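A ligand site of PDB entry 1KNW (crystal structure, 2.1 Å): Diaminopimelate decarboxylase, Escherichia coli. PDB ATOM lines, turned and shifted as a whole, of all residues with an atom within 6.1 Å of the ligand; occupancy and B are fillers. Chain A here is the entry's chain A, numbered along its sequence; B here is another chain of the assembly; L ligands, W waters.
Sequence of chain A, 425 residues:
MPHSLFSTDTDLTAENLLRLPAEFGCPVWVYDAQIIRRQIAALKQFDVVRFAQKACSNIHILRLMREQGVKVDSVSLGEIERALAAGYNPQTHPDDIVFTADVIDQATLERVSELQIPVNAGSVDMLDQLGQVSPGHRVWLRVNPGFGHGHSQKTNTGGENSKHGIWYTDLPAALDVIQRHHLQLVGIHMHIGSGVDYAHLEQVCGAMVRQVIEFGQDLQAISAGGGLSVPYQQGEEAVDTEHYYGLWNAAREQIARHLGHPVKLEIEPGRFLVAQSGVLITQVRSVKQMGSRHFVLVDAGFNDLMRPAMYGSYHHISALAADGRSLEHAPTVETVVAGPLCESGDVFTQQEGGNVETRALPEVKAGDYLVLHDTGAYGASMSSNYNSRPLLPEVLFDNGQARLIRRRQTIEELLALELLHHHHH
Water W4 lies within hydrogen-bond range of O4 of the ligand (2.6 Å), NE of Arg 271 (2.9 Å) and O of Leu 228 (3.0 Å).
Water W3 lies within hydrogen-bond range of O5 of the ligand (2.6 Å), O of Leu 228 (2.7 Å) and N of Phe 272 (2.9 Å).
Water W5 lies within hydrogen-bond range of O4 of the ligand (2.8 Å) and NE2 of His 191 (3.5 Å).
Water W2 bridges NH2 of Arg 271 (2.7 Å) and O4 of the ligand (2.8 Å).
Water W6 lies within hydrogen-bond range of an oxygen (O1) of the ligand (2.8 Å), the guanidinium group of Arg 142 (2.8 Å) and the side-chain sulfur of Cys 342 of chain B (3.5 Å).
CB of Ala 52 touches C8 of the ligand (3.3 Å).
Asp 73 touches the ligand.
Thr 100 touches the ligand (CG2 to C2, 3.7 Å).
His 191 touches the ligand.
Gly 226 touches the ligand (CA to O5, 3.8 Å).
C of Pro 269 touches O5 of the ligand (3.9 Å).
Hydrophobic or aromatic side chains that line the ligand: Ala 52, His 191 and Tyr 378.
Of the 25 residues printed, 13 come within 4 Å of the ligand.
Along chain A the residues within 4 Å of the ligand span positions 52 to 378.
The backbone carbonyl oxygen (O) of Glu 268 sits close to the backbone NH (N) of Gly 226, 3.5 Å away.
The backbone carbonyl oxygen (O) of Pro 269 lies within hydrogen-bond range of the backbone NH (N) of Ala 52.
The side-chain sulfur (SG) of Cys 342 of chain B sits at hydrogen-bond distance from the backbone carbonyl oxygen (O) of Thr 100 (3.4 Å).
The side-chain amino group (NZ) of Lys 54 lies within hydrogen-bond range of the backbone carbonyl oxygen (O) of Cys 342 of chain B, at 2.9 Å.
A ring nitrogen (ND1) of His 191 sits at hydrogen-bond distance from the backbone NH of Gly 226 (2.8 Å).
N of Tyr 378 lies within hydrogen-bond range of O of Ala 55 (2.9 Å).
The side-chain hydroxyl (OG1) of Thr 100 is in hydrogen-bond range of the side-chain carboxylate (OD1) of Asp 73 (2.6 Å).
O of His 191 lies within hydrogen-bond range of NH2 of Arg 142 (2.9 Å).
The side-chain amino group (NZ) of Lys 54 is covalently linked to a carbon (C5) of the ligand (1.3 Å).
The backbone NH (N) of Gly 270 lies within hydrogen-bond range of an oxygen (O5) of the ligand, at 3.0 Å.
The backbone carbonyl oxygen (O) of Cys 342 of chain B sits close to an oxygen (O1) of the ligand, 3.3 Å away.
N of Gly 227 lies within hydrogen-bond range of O5 of the ligand, at 2.8 Å.
An oxygen (O3) of the ligand is in hydrogen-bond range of the side-chain hydroxyl (OH) of Tyr 378, at 2.6 Å.
The side-chain carboxylate (OE2) of Glu 268 sits at hydrogen-bond distance from a nitrogen (N1) of the ligand.
O3 of the ligand sits at hydrogen-bond distance from N of Arg 271, 2.8 Å away.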
ATOM      1  N   ALA A  52      20.984   6.098  12.229  1.00  0.00           N
ATOM      2  CA  ALA A  52      20.709   6.850  10.991  1.00  0.00           C
ATOM      3  C   ALA A  52      20.039   8.147  11.382  1.00  0.00           C
ATOM      4  O   ALA A  52      18.822   8.198  11.564  1.00  0.00           O
ATOM      5  CB  ALA A  52      19.770   6.012  10.116  1.00  0.00           C
ATOM      6  N   LYS A  54      19.058  10.790  10.085  1.00  0.00           N
ATOM      7  CA  LYS A  54      18.010  11.431   9.289  1.00  0.00           C
ATOM      8  C   LYS A  54      16.629  11.155   9.850  1.00  0.00           C
ATOM      9  O   LYS A  54      15.658  11.882   9.546  1.00  0.00           O
ATOM     10  CB  LYS A  54      18.091  11.084   7.811  1.00  0.00           C
ATOM     11  CG  LYS A  54      17.618   9.668   7.454  1.00  0.00           C
ATOM     12  CD  LYS A  54      17.079   9.632   6.036  1.00  0.00           C
ATOM     13  CE  LYS A  54      16.367   8.360   5.668  1.00  0.00           C
ATOM     14  NZ  LYS A  54      17.336   7.226   5.496  1.00  0.00           N
ATOM     15  N   ALA A  55      16.484  10.143  10.701  1.00  0.00           N
ATOM     16  CA  ALA A  55      15.206   9.857  11.336  1.00  0.00           C
ATOM     17  C   ALA A  55      14.846  10.831  12.452  1.00  0.00           C
ATOM     18  O   ALA A  55      13.660  11.025  12.726  1.00  0.00           O
ATOM     19  CB  ALA A  55      15.206   8.432  11.895  1.00  0.00           C
ATOM     20  N   ASP A  73      25.484   7.731  11.546  1.00  0.00           N
ATOM     21  CA  ASP A  73      25.618   7.831  10.101  1.00  0.00           C
ATOM     22  C   ASP A  73      25.101   9.215   9.653  1.00  0.00           C
ATOM     23  O   ASP A  73      23.920   9.467   9.892  1.00  0.00           O
ATOM     24  CB  ASP A  73      24.772   6.749   9.396  1.00  0.00           C
ATOM     25  CG  ASP A  73      25.192   6.636   7.926  1.00  0.00           C
ATOM     26  OD1 ASP A  73      26.410   6.750   7.688  1.00  0.00           O
ATOM     27  OD2 ASP A  73      24.318   6.481   7.066  1.00  0.00           O
ATOM     28  N   VAL A  75      24.262  11.784   6.352  1.00  0.00           N
ATOM     29  CA  VAL A  75      23.984  11.668   4.927  1.00  0.00           C
ATOM     30  C   VAL A  75      24.065  12.994   4.201  1.00  0.00           C
ATOM     31  O   VAL A  75      23.763  13.105   3.005  1.00  0.00           O
ATOM     32  CB  VAL A  75      22.660  10.961   4.640  1.00  0.00           C
ATOM     33  CG1 VAL A  75      22.688   9.568   5.297  1.00  0.00           C
ATOM     34  CG2 VAL A  75      21.466  11.745   5.135  1.00  0.00           C
ATOM     35  N   THR A 100      27.538   8.893   4.462  1.00  0.00           N
ATOM     36  CA  THR A 100      26.921   7.962   3.528  1.00  0.00           C
ATOM     37  C   THR A 100      25.990   8.679   2.547  1.00  0.00           C
ATOM     38  O   THR A 100      25.067   9.379   2.977  1.00  0.00           O
ATOM     39  CB  THR A 100      26.076   6.915   4.313  1.00  0.00           C
ATOM     40  OG1 THR A 100      26.965   6.207   5.202  1.00  0.00           O
ATOM     41  CG2 THR A 100      25.404   5.940   3.379  1.00  0.00           C
ATOM     42  N   ASN A 120      31.084   6.268   2.902  1.00  0.00           N
ATOM     43  CA  ASN A 120      30.363   5.150   2.311  1.00  0.00           C
ATOM     44  C   ASN A 120      29.767   5.638   0.976  1.00  0.00           C
ATOM     45  O   ASN A 120      28.839   6.451   0.964  1.00  0.00           O
ATOM     46  CB  ASN A 120      29.245   4.695   3.258  1.00  0.00           C
ATOM     47  CG  ASN A 120      28.341   3.644   2.683  1.00  0.00           C
ATOM     48  OD1 ASN A 120      28.359   3.344   1.494  1.00  0.00           O
ATOM     49  ND2 ASN A 120      27.459   3.071   3.530  1.00  0.00           N
ATOM     50  N   ARG A 142      28.465   1.068  -0.619  1.00  0.00           N
ATOM     51  CA  ARG A 142      27.064   0.663  -0.519  1.00  0.00           C
ATOM     52  C   ARG A 142      26.695  -0.084  -1.811  1.00  0.00           C
ATOM     53  O   ARG A 142      26.805   0.473  -2.903  1.00  0.00           O
ATOM     54  CB  ARG A 142      26.114   1.811  -0.280  1.00  0.00           C
ATOM     55  CG  ARG A 142      24.631   1.382  -0.351  1.00  0.00           C
ATOM     56  CD  ARG A 142      23.694   2.546  -0.102  1.00  0.00           C
ATOM     57  NE  ARG A 142      22.282   2.088  -0.038  1.00  0.00           N
ATOM     58  CZ  ARG A 142      21.286   2.920   0.229  1.00  0.00           C
ATOM     59  NH1 ARG A 142      21.555   4.217   0.441  1.00  0.00           N
ATOM     60  NH2 ARG A 142      20.033   2.511   0.291  1.00  0.00           N
ATOM     61  N   HIS A 164      19.899   4.216  -5.312  1.00  0.00           N
ATOM     62  CA  HIS A 164      20.810   3.920  -4.239  1.00  0.00           C
ATOM     63  C   HIS A 164      21.852   2.858  -4.513  1.00  0.00           C
ATOM     64  O   HIS A 164      21.528   1.715  -4.842  1.00  0.00           O
ATOM     65  CB  HIS A 164      19.986   3.446  -2.998  1.00  0.00           C
ATOM     66  CG  HIS A 164      19.122   4.546  -2.448  1.00  0.00           C
ATOM     67  ND1 HIS A 164      19.615   5.776  -2.101  1.00  0.00           N
ATOM     68  CD2 HIS A 164      17.796   4.560  -2.154  1.00  0.00           C
ATOM     69  CE1 HIS A 164      18.624   6.521  -1.632  1.00  0.00           C
ATOM     70  NE2 HIS A 164      17.520   5.804  -1.641  1.00  0.00           N
ATOM     71  N   HIS A 189      28.470  -2.378   2.604  1.00  0.00           N
ATOM     72  CA  HIS A 189      27.192  -2.051   3.277  1.00  0.00           C
ATOM     73  C   HIS A 189      26.035  -2.245   2.322  1.00  0.00           C
ATOM     74  O   HIS A 189      26.181  -2.113   1.111  1.00  0.00           O
ATOM     75  CB  HIS A 189      27.308  -0.591   3.734  1.00  0.00           C
ATOM     76  CG  HIS A 189      26.046   0.183   3.861  1.00  0.00           C
ATOM     77  ND1 HIS A 189      25.563   0.643   5.083  1.00  0.00           N
ATOM     78  CD2 HIS A 189      25.217   0.724   2.931  1.00  0.00           C
ATOM     79  CE1 HIS A 189      24.470   1.356   4.894  1.00  0.00           C
ATOM     80  NE2 HIS A 189      24.245   1.419   3.588  1.00  0.00           N
ATOM     81  N   HIS A 191      21.738  -1.094   2.400  1.00  0.00           N
ATOM     82  CA  HIS A 191      20.560  -0.547   3.086  1.00  0.00           C
ATOM     83  C   HIS A 191      19.339  -0.763   2.190  1.00  0.00           C
ATOM     84  O   HIS A 191      19.173  -0.148   1.138  1.00  0.00           O
ATOM     85  CB  HIS A 191      20.736   0.909   3.458  1.00  0.00           C
ATOM     86  CG  HIS A 191      19.488   1.534   4.030  1.00  0.00           C
ATOM     87  ND1 HIS A 191      18.895   1.063   5.194  1.00  0.00           N
ATOM     88  CD2 HIS A 191      18.639   2.452   3.507  1.00  0.00           C
ATOM     89  CE1 HIS A 191      17.755   1.721   5.382  1.00  0.00           C
ATOM     90  NE2 HIS A 191      17.595   2.584   4.392  1.00  0.00           N
ATOM     91  N   GLY A 225      22.672  -2.203   7.334  1.00  0.00           N
ATOM     92  CA  GLY A 225      21.814  -1.064   6.947  1.00  0.00           C
ATOM     93  C   GLY A 225      20.679  -0.944   7.963  1.00  0.00           C
ATOM     94  O   GLY A 225      20.816  -1.412   9.112  1.00  0.00           O
ATOM     95  N   GLY A 226      19.610  -0.270   7.577  1.00  0.00           N
ATOM     96  CA  GLY A 226      18.486  -0.076   8.510  1.00  0.00           C
ATOM     97  C   GLY A 226      17.223  -0.716   7.963  1.00  0.00           C
ATOM     98  O   GLY A 226      17.279  -1.732   7.251  1.00  0.00           O
ATOM     99  N   GLY A 227      16.072  -0.148   8.310  1.00  0.00           N
ATOM    100  CA  GLY A 227      14.816  -0.672   7.807  1.00  0.00           C
ATOM    101  C   GLY A 227      14.108  -1.595   8.777  1.00  0.00           C
ATOM    102  O   GLY A 227      13.173  -2.299   8.377  1.00  0.00           O
ATOM    103  N   LEU A 228      14.513  -1.616  10.032  1.00  0.00           N
ATOM    104  CA  LEU A 228      13.723  -2.337  11.062  1.00  0.00           C
ATOM    105  C   LEU A 228      12.404  -1.550  11.204  1.00  0.00           C
ATOM    106  O   LEU A 228      12.445  -0.320  11.198  1.00  0.00           O
ATOM    107  CB  LEU A 228      14.434  -2.336  12.396  1.00  0.00           C
ATOM    108  CG  LEU A 228      15.582  -3.320  12.622  1.00  0.00           C
ATOM    109  CD1 LEU A 228      16.766  -3.018  11.707  1.00  0.00           C
ATOM    110  CD2 LEU A 228      16.021  -3.283  14.078  1.00  0.00           C
ATOM    111  N   GLU A 268      22.318  -0.370  11.228  1.00  0.00           N
ATOM    112  CA  GLU A 268      22.124   1.082  11.073  1.00  0.00           C
ATOM    113  C   GLU A 268      20.682   1.509  11.125  1.00  0.00           C
ATOM    114  O   GLU A 268      20.144   2.045  10.142  1.00  0.00           O
ATOM    115  CB  GLU A 268      22.723   1.415   9.676  1.00  0.00           C
ATOM    116  CG  GLU A 268      23.060   2.850   9.403  1.00  0.00           C
ATOM    117  CD  GLU A 268      23.820   3.000   8.081  1.00  0.00           C
ATOM    118  OE1 GLU A 268      25.064   3.148   8.133  1.00  0.00           O
ATOM    119  OE2 GLU A 268      23.181   2.846   7.015  1.00  0.00           O
ATOM    120  N   PRO A 269      20.015   1.338  12.262  1.00  0.00           N
ATOM    121  CA  PRO A 269      18.621   1.667  12.418  1.00  0.00           C
ATOM    122  C   PRO A 269      18.408   3.179  12.512  1.00  0.00           C
ATOM    123  O   PRO A 269      19.246   3.900  13.047  1.00  0.00           O
ATOM    124  CB  PRO A 269      18.246   1.050  13.778  1.00  0.00           C
ATOM    125  CG  PRO A 269      19.525   1.115  14.556  1.00  0.00           C
ATOM    126  CD  PRO A 269      20.621   0.904  13.541  1.00  0.00           C
ATOM    127  N   GLY A 270      17.285   3.618  11.993  1.00  0.00           N
ATOM    128  CA  GLY A 270      16.880   5.033  12.117  1.00  0.00           C
ATOM    129  C   GLY A 270      15.537   4.999  12.904  1.00  0.00           C
ATOM    130  O   GLY A 270      15.529   5.026  14.121  1.00  0.00           O
ATOM    131  N   ARG A 271      14.494   4.632  12.174  1.00  0.00           N
ATOM    132  CA  ARG A 271      13.168   4.514  12.750  1.00  0.00           C
ATOM    133  C   ARG A 271      13.131   3.721  14.049  1.00  0.00           C
ATOM    134  O   ARG A 271      12.430   4.109  14.996  1.00  0.00           O
ATOM    135  CB  ARG A 271      12.233   3.855  11.720  1.00  0.00           C
ATOM    136  CG  ARG A 271      10.742   3.992  12.082  1.00  0.00           C
ATOM    137  CD  ARG A 271       9.931   3.075  11.129  1.00  0.00           C
ATOM    138  NE  ARG A 271      10.135   3.455   9.746  1.00  0.00           N
ATOM    139  CZ  ARG A 271       9.444   4.338   9.067  1.00  0.00           C
ATOM    140  NH1 ARG A 271       8.425   5.016   9.619  1.00  0.00           N
ATOM    141  NH2 ARG A 271       9.726   4.571   7.781  1.00  0.00           N
ATOM    142  N   PHE A 272      13.677   2.514  14.044  1.00  0.00           N
ATOM    143  CA  PHE A 272      13.563   1.592  15.166  1.00  0.00           C
ATOM    144  C   PHE A 272      13.973   2.227  16.487  1.00  0.00           C
ATOM    145  O   PHE A 272      13.336   1.952  17.511  1.00  0.00           O
ATOM    146  CB  PHE A 272      14.345   0.315  14.924  1.00  0.00           C
ATOM    147  CG  PHE A 272      14.299  -0.682  16.053  1.00  0.00           C
ATOM    148  CD1 PHE A 272      13.246  -1.583  16.164  1.00  0.00           C
ATOM    149  CD2 PHE A 272      15.324  -0.751  16.982  1.00  0.00           C
ATOM    150  CE1 PHE A 272      13.211  -2.519  17.180  1.00  0.00           C
ATOM    151  CE2 PHE A 272      15.314  -1.688  17.998  1.00  0.00           C
ATOM    152  CZ  PHE A 272      14.249  -2.585  18.088  1.00  0.00           C
ATOM    153  N   ALA A 377      10.328   9.247  14.711  1.00  0.00           N
ATOM    154  CA  ALA A 377      11.096   9.056  13.487  1.00  0.00           C
ATOM    155  C   ALA A 377      10.367   9.711  12.312  1.00  0.00           C
ATOM    156  O   ALA A 377       9.172   9.510  12.111  1.00  0.00           O
ATOM    157  CB  ALA A 377      11.254   7.558  13.185  1.00  0.00           C
ATOM    158  N   TYR A 378      11.119  10.466  11.527  1.00  0.00           N
ATOM    159  CA  TYR A 378      10.612  11.125  10.347  1.00  0.00           C
ATOM    160  C   TYR A 378       9.466  12.076  10.667  1.00  0.00           C
ATOM    161  O   TYR A 378       8.530  12.240   9.889  1.00  0.00           O
ATOM    162  CB  TYR A 378      10.205  10.088   9.279  1.00  0.00           C
ATOM    163  CG  TYR A 378      11.398   9.177   8.945  1.00  0.00           C
ATOM    164  CD1 TYR A 378      11.443   7.877   9.380  1.00  0.00           C
ATOM    165  CD2 TYR A 378      12.536   9.723   8.355  1.00  0.00           C
ATOM    166  CE1 TYR A 378      12.555   7.080   9.151  1.00  0.00           C
ATOM    167  CE2 TYR A 378      13.661   8.941   8.135  1.00  0.00           C
ATOM    168  CZ  TYR A 378      13.661   7.626   8.531  1.00  0.00           C
ATOM    169  OH  TYR A 378      14.786   6.858   8.342  1.00  0.00           O
ATOM    170  N   CYS B 342      19.362  10.630   1.123  1.00  0.00           N
ATOM    171  CA  CYS B 342      19.421   9.193   1.447  1.00  0.00           C
ATOM    172  C   CYS B 342      18.005   8.728   1.788  1.00  0.00           C
ATOM    173  O   CYS B 342      17.621   8.629   2.946  1.00  0.00           O
ATOM    174  CB  CYS B 342      20.431   8.907   2.525  1.00  0.00           C
ATOM    175  SG  CYS B 342      22.042   8.357   1.884  1.00  0.00           S
ATOM    176  N   GLU B 343      17.196   8.674   0.751  1.00  0.00           N
ATOM    177  CA  GLU B 343      15.746   8.508   0.838  1.00  0.00           C
ATOM    178  C   GLU B 343      15.240   7.957  -0.497  1.00  0.00           C
ATOM    179  O   GLU B 343      15.480   8.582  -1.553  1.00  0.00           O
ATOM    180  CB  GLU B 343      15.116   9.872   1.140  1.00  0.00           C
ATOM    181  CG  GLU B 343      13.644   9.999   0.802  1.00  0.00           C
ATOM    182  CD  GLU B 343      12.757   9.074   1.615  1.00  0.00           C
ATOM    183  OE1 GLU B 343      12.981   8.968   2.845  1.00  0.00           O
ATOM    184  OE2 GLU B 343      11.849   8.458   1.027  1.00  0.00           O
ATOM    185  N   TYR B 386      14.762  18.422   5.312  1.00  0.00           N
ATOM    186  CA  TYR B 386      15.008  16.978   5.385  1.00  0.00           C
ATOM    187  C   TYR B 386      16.448  16.631   5.043  1.00  0.00           C
ATOM    188  O   TYR B 386      17.026  17.162   4.093  1.00  0.00           O
ATOM    189  CB  TYR B 386      14.025  16.214   4.503  1.00  0.00           C
ATOM    190  CG  TYR B 386      14.007  14.722   4.667  1.00  0.00           C
ATOM    191  CD1 TYR B 386      14.180  14.100   5.897  1.00  0.00           C
ATOM    192  CD2 TYR B 386      13.792  13.900   3.556  1.00  0.00           C
ATOM    193  CE1 TYR B 386      14.166  12.723   6.026  1.00  0.00           C
ATOM    194  CE2 TYR B 386      13.758  12.519   3.677  1.00  0.00           C
ATOM    195  CZ  TYR B 386      13.938  11.944   4.906  1.00  0.00           C
ATOM    196  OH  TYR B 386      13.888  10.570   5.028  1.00  0.00           O
HETATM  197  N1  LIG L   1      20.904   3.818   6.460  1.00  0.00           N
HETATM  198  C1  LIG L   1      20.852   4.757   5.462  1.00  0.00           C
HETATM  199  C2  LIG L   1      22.065   4.861   4.523  1.00  0.00           C
HETATM  200  C3  LIG L   1      19.691   5.513   5.327  1.00  0.00           C
HETATM  201  O1  LIG L   1      19.562   6.359   4.364  1.00  0.00           O
HETATM  202  C4  LIG L   1      18.606   5.356   6.250  1.00  0.00           C
HETATM  203  C5  LIG L   1      17.382   6.166   6.270  1.00  0.00           C
HETATM  204  C6  LIG L   1      18.753   4.388   7.290  1.00  0.00           C
HETATM  205  C7  LIG L   1      19.919   3.615   7.373  1.00  0.00           C
HETATM  206  C8  LIG L   1      17.659   4.206   8.317  1.00  0.00           C
HETATM  207  O2  LIG L   1      16.464   3.697   7.718  1.00  0.00           O
HETATM  208  P1  LIG L   1      15.277   3.281   8.746  1.00  0.00           P
HETATM  209  O3  LIG L   1      14.804   4.525   9.430  1.00  0.00           O
HETATM  210  O4  LIG L   1      14.172   2.641   7.954  1.00  0.00           O
HETATM  211  O5  LIG L   1      15.843   2.312   9.730  1.00  0.00           O
HETATM  212  O   HOH W   1      21.532   7.112   7.488  1.00  0.00           O
HETATM  213  O   HOH W   2      12.096   3.942   6.594  1.00  0.00           O
HETATM  214  O   HOH W   3      14.660   1.139  11.727  1.00  0.00           O
HETATM  215  O   HOH W   4      12.032   1.495   8.863  1.00  0.00           O
HETATM  216  O   HOH W   5      14.349   1.760   5.337  1.00  0.00           O
HETATM  217  O   HOH W   6      19.573   5.877   1.595  1.00  0.00           O
